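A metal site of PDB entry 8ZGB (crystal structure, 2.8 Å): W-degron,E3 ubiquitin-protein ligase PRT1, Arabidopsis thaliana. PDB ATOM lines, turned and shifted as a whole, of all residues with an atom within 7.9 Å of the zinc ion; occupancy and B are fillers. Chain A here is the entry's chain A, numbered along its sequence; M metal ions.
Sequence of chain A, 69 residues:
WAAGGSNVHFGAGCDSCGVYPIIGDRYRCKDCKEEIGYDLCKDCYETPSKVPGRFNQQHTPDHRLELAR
SG of Cys 41 sits close to N of Asp 43 (3.8 Å).
The side-chain sulfur (SG) of Cys 14 sits close to the backbone NH (N) of Ser 16 (3.5 Å).
O of Val 19 is in hydrogen-bond range of N of Cys 14, 3.3 Å away.
OG of Ser 16 lies close to SG of Cys 44.
The backbone NH (N) of Val 19 sits close to the side-chain sulfur (SG) of Cys 17, 3.6 Å away.
O of Cys 44 is in hydrogen-bond range of OG1 of Thr 47 (3.1 Å).
O of Cys 14 lies within hydrogen-bond range of NE of Arg 54 (3.4 Å).
Of the 17 residues printed, 4 come within 4 Å of the zinc ion.
The zinc ion is bound by SG of Cys 17 (2.3 Å), SG of Cys 44 (2.3 Å), SG of Cys 14 (2.3 Å) and SG of Cys 41 (2.3 Å).
The zinc ion has four donor atoms within binding distance.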
ATOM      1  N   GLY A  13      -4.436   6.078  20.464  1.00  0.00           N
ATOM      2  CA  GLY A  13      -3.505   5.092  19.962  1.00  0.00           C
ATOM      3  C   GLY A  13      -3.743   3.755  20.636  1.00  0.00           C
ATOM      4  O   GLY A  13      -4.307   3.672  21.721  1.00  0.00           O
ATOM      5  N   CYS A  14      -3.306   2.693  19.964  1.00  0.00           N
ATOM      6  CA  CYS A  14      -3.520   1.349  20.474  1.00  0.00           C
ATOM      7  C   CYS A  14      -2.615   1.073  21.683  1.00  0.00           C
ATOM      8  O   CYS A  14      -1.414   1.342  21.644  1.00  0.00           O
ATOM      9  CB  CYS A  14      -3.233   0.344  19.381  1.00  0.00           C
ATOM     10  SG  CYS A  14      -3.657  -1.413  19.748  1.00  0.00           S
ATOM     11  N   ASP A  15      -3.210   0.568  22.751  1.00  0.00           N
ATOM     12  CA  ASP A  15      -2.453   0.201  23.940  1.00  0.00           C
ATOM     13  C   ASP A  15      -1.670  -1.093  23.790  1.00  0.00           C
ATOM     14  O   ASP A  15      -0.830  -1.395  24.641  1.00  0.00           O
ATOM     15  CB  ASP A  15      -3.362   0.087  25.150  1.00  0.00           C
ATOM     16  CG  ASP A  15      -3.809   1.420  25.689  1.00  0.00           C
ATOM     17  OD1 ASP A  15      -4.798   1.975  25.181  1.00  0.00           O
ATOM     18  OD2 ASP A  15      -3.189   1.911  26.633  1.00  0.00           O
ATOM     19  N   SER A  16      -1.931  -1.879  22.741  1.00  0.00           N
ATOM     20  CA  SER A  16      -1.276  -3.166  22.561  1.00  0.00           C
ATOM     21  C   SER A  16      -0.075  -3.080  21.616  1.00  0.00           C
ATOM     22  O   SER A  16       1.024  -3.511  21.974  1.00  0.00           O
ATOM     23  CB  SER A  16      -2.274  -4.206  22.040  1.00  0.00           C
ATOM     24  OG  SER A  16      -1.611  -5.408  21.655  1.00  0.00           O
ATOM     25  N   CYS A  17      -0.268  -2.530  20.422  1.00  0.00           N
ATOM     26  CA  CYS A  17       0.772  -2.467  19.414  1.00  0.00           C
ATOM     27  C   CYS A  17       1.354  -1.090  19.223  1.00  0.00           C
ATOM     28  O   CYS A  17       2.288  -0.930  18.425  1.00  0.00           O
ATOM     29  CB  CYS A  17       0.229  -2.990  18.074  1.00  0.00           C
ATOM     30  SG  CYS A  17      -1.090  -1.890  17.367  1.00  0.00           S
ATOM     31  N   GLY A  18       0.829  -0.080  19.915  1.00  0.00           N
ATOM     32  CA  GLY A  18       1.358   1.260  19.837  1.00  0.00           C
ATOM     33  C   GLY A  18       1.118   1.988  18.545  1.00  0.00           C
ATOM     34  O   GLY A  18       1.698   3.065  18.341  1.00  0.00           O
ATOM     35  N   VAL A  19       0.281   1.462  17.653  1.00  0.00           N
ATOM     36  CA  VAL A  19       0.075   2.130  16.375  1.00  0.00           C
ATOM     37  C   VAL A  19      -0.552   3.485  16.609  1.00  0.00           C
ATOM     38  O   VAL A  19      -1.404   3.657  17.480  1.00  0.00           O
ATOM     39  CB  VAL A  19      -0.805   1.285  15.445  1.00  0.00           C
ATOM     40  CG1 VAL A  19      -2.181   1.162  16.017  1.00  0.00           C
ATOM     41  CG2 VAL A  19      -0.855   1.909  14.063  1.00  0.00           C
ATOM     42  N   ILE A  22      -4.779   5.406  14.971  1.00  0.00           N
ATOM     43  CA  ILE A  22      -5.461   4.139  14.764  1.00  0.00           C
ATOM     44  C   ILE A  22      -6.112   4.204  13.398  1.00  0.00           C
ATOM     45  O   ILE A  22      -7.074   4.949  13.188  1.00  0.00           O
ATOM     46  CB  ILE A  22      -6.504   3.873  15.863  1.00  0.00           C
ATOM     47  CG1 ILE A  22      -5.793   3.644  17.197  1.00  0.00           C
ATOM     48  CG2 ILE A  22      -7.365   2.689  15.491  1.00  0.00           C
ATOM     49  CD1 ILE A  22      -6.746   3.350  18.345  1.00  0.00           C
ATOM     50  N   ASP A  39      -7.682   2.038  24.623  1.00  0.00           N
ATOM     51  CA  ASP A  39      -8.144   1.871  23.255  1.00  0.00           C
ATOM     52  C   ASP A  39      -7.288   0.832  22.587  1.00  0.00           C
ATOM     53  O   ASP A  39      -6.120   0.648  22.944  1.00  0.00           O
ATOM     54  CB  ASP A  39      -8.108   3.207  22.469  1.00  0.00           C
ATOM     55  CG  ASP A  39      -8.777   4.334  23.239  1.00  0.00           C
ATOM     56  OD1 ASP A  39     -10.018   4.297  23.408  1.00  0.00           O
ATOM     57  OD2 ASP A  39      -8.069   5.258  23.666  1.00  0.00           O
ATOM     58  N   LEU A  40      -7.856   0.158  21.587  1.00  0.00           N
ATOM     59  CA  LEU A  40      -7.114  -0.797  20.772  1.00  0.00           C
ATOM     60  C   LEU A  40      -7.655  -0.796  19.343  1.00  0.00           C
ATOM     61  O   LEU A  40      -8.827  -0.495  19.101  1.00  0.00           O
ATOM     62  CB  LEU A  40      -7.225  -2.208  21.368  1.00  0.00           C
ATOM     63  CG  LEU A  40      -6.468  -2.446  22.667  1.00  0.00           C
ATOM     64  CD1 LEU A  40      -6.517  -3.924  23.032  1.00  0.00           C
ATOM     65  CD2 LEU A  40      -4.994  -2.004  22.580  1.00  0.00           C
ATOM     66  N   CYS A  41      -6.781  -1.103  18.396  1.00  0.00           N
ATOM     67  CA  CYS A  41      -7.195  -1.284  17.023  1.00  0.00           C
ATOM     68  C   CYS A  41      -7.856  -2.658  16.837  1.00  0.00           C
ATOM     69  O   CYS A  41      -7.900  -3.499  17.748  1.00  0.00           O
ATOM     70  CB  CYS A  41      -6.006  -1.143  16.097  1.00  0.00           C
ATOM     71  SG  CYS A  41      -4.869  -2.482  16.162  1.00  0.00           S
ATOM     72  N   LYS A  42      -8.373  -2.883  15.639  1.00  0.00           N
ATOM     73  CA  LYS A  42      -9.112  -4.114  15.367  1.00  0.00           C
ATOM     74  C   LYS A  42      -8.221  -5.341  15.463  1.00  0.00           C
ATOM     75  O   LYS A  42      -8.619  -6.361  16.041  1.00  0.00           O
ATOM     76  CB  LYS A  42      -9.739  -4.064  13.971  1.00  0.00           C
ATOM     77  CG  LYS A  42     -10.722  -5.194  13.689  1.00  0.00           C
ATOM     78  CD  LYS A  42     -11.636  -4.955  12.505  1.00  0.00           C
ATOM     79  CE  LYS A  42     -12.545  -6.165  12.265  1.00  0.00           C
ATOM     80  NZ  LYS A  42     -13.536  -6.537  13.283  1.00  0.00           N
ATOM     81  N   ASP A  43      -7.032  -5.296  14.853  1.00  0.00           N
ATOM     82  CA  ASP A  43      -6.166  -6.462  14.925  1.00  0.00           C
ATOM     83  C   ASP A  43      -5.912  -6.836  16.378  1.00  0.00           C
ATOM     84  O   ASP A  43      -6.060  -8.006  16.763  1.00  0.00           O
ATOM     85  CB  ASP A  43      -4.865  -6.195  14.187  1.00  0.00           C
ATOM     86  CG  ASP A  43      -5.050  -6.245  12.679  1.00  0.00           C
ATOM     87  OD1 ASP A  43      -6.212  -6.372  12.223  1.00  0.00           O
ATOM     88  OD2 ASP A  43      -4.049  -6.192  11.952  1.00  0.00           O
ATOM     89  N   CYS A  44      -5.566  -5.853  17.213  1.00  0.00           N
ATOM     90  CA  CYS A  44      -5.316  -6.130  18.630  1.00  0.00           C
ATOM     91  C   CYS A  44      -6.591  -6.513  19.360  1.00  0.00           C
ATOM     92  O   CYS A  44      -6.547  -7.345  20.284  1.00  0.00           O
ATOM     93  CB  CYS A  44      -4.674  -4.920  19.275  1.00  0.00           C
ATOM     94  SG  CYS A  44      -2.921  -4.666  18.778  1.00  0.00           S
ATOM     95  N   TYR A  45      -7.746  -5.970  18.935  1.00  0.00           N
ATOM     96  CA  TYR A  45      -9.017  -6.418  19.489  1.00  0.00           C
ATOM     97  C   TYR A  45      -9.239  -7.901  19.186  1.00  0.00           C
ATOM     98  O   TYR A  45      -9.616  -8.683  20.067  1.00  0.00           O
ATOM     99  CB  TYR A  45     -10.168  -5.594  18.926  1.00  0.00           C
ATOM    100  CG  TYR A  45     -11.557  -6.065  19.328  1.00  0.00           C
ATOM    101  CD1 TYR A  45     -12.082  -5.784  20.582  1.00  0.00           C
ATOM    102  CD2 TYR A  45     -12.343  -6.791  18.429  1.00  0.00           C
ATOM    103  CE1 TYR A  45     -13.355  -6.205  20.931  1.00  0.00           C
ATOM    104  CE2 TYR A  45     -13.615  -7.212  18.778  1.00  0.00           C
ATOM    105  CZ  TYR A  45     -14.114  -6.912  20.023  1.00  0.00           C
ATOM    106  OH  TYR A  45     -15.380  -7.343  20.366  1.00  0.00           O
ATOM    107  N   THR A  47      -7.168 -10.236  18.383  1.00  0.00           N
ATOM    108  CA  THR A  47      -6.150 -11.179  18.842  1.00  0.00           C
ATOM    109  C   THR A  47      -6.242 -11.336  20.356  1.00  0.00           C
ATOM    110  O   THR A  47      -6.299 -10.321  21.069  1.00  0.00           O
ATOM    111  CB  THR A  47      -4.747 -10.678  18.481  1.00  0.00           C
ATOM    112  OG1 THR A  47      -4.604  -9.314  18.905  1.00  0.00           O
ATOM    113  CG2 THR A  47      -4.504 -10.780  16.993  1.00  0.00           C
ATOM    114  N   ARG A  54      -0.780   0.756  28.416  1.00  0.00           N
ATOM    115  CA  ARG A  54       0.514   1.317  28.046  1.00  0.00           C
ATOM    116  C   ARG A  54       0.831   2.530  28.908  1.00  0.00           C
ATOM    117  O   ARG A  54       1.976   3.008  28.905  1.00  0.00           O
ATOM    118  CB  ARG A  54       0.529   1.746  26.579  1.00  0.00           C
ATOM    119  CG  ARG A  54       1.190   0.773  25.643  1.00  0.00           C
ATOM    120  CD  ARG A  54       1.090   1.295  24.197  1.00  0.00           C
ATOM    121  NE  ARG A  54       1.422   0.263  23.220  1.00  0.00           N
ATOM    122  CZ  ARG A  54       2.653  -0.015  22.808  1.00  0.00           C
ATOM    123  NH1 ARG A  54       3.699   0.668  23.276  1.00  0.00           N
ATOM    124  NH2 ARG A  54       2.831  -0.993  21.918  1.00  0.00           N
HETATM  125 ZN    ZN M   1      -3.225  -2.595  17.810  1.00  0.00          ZN
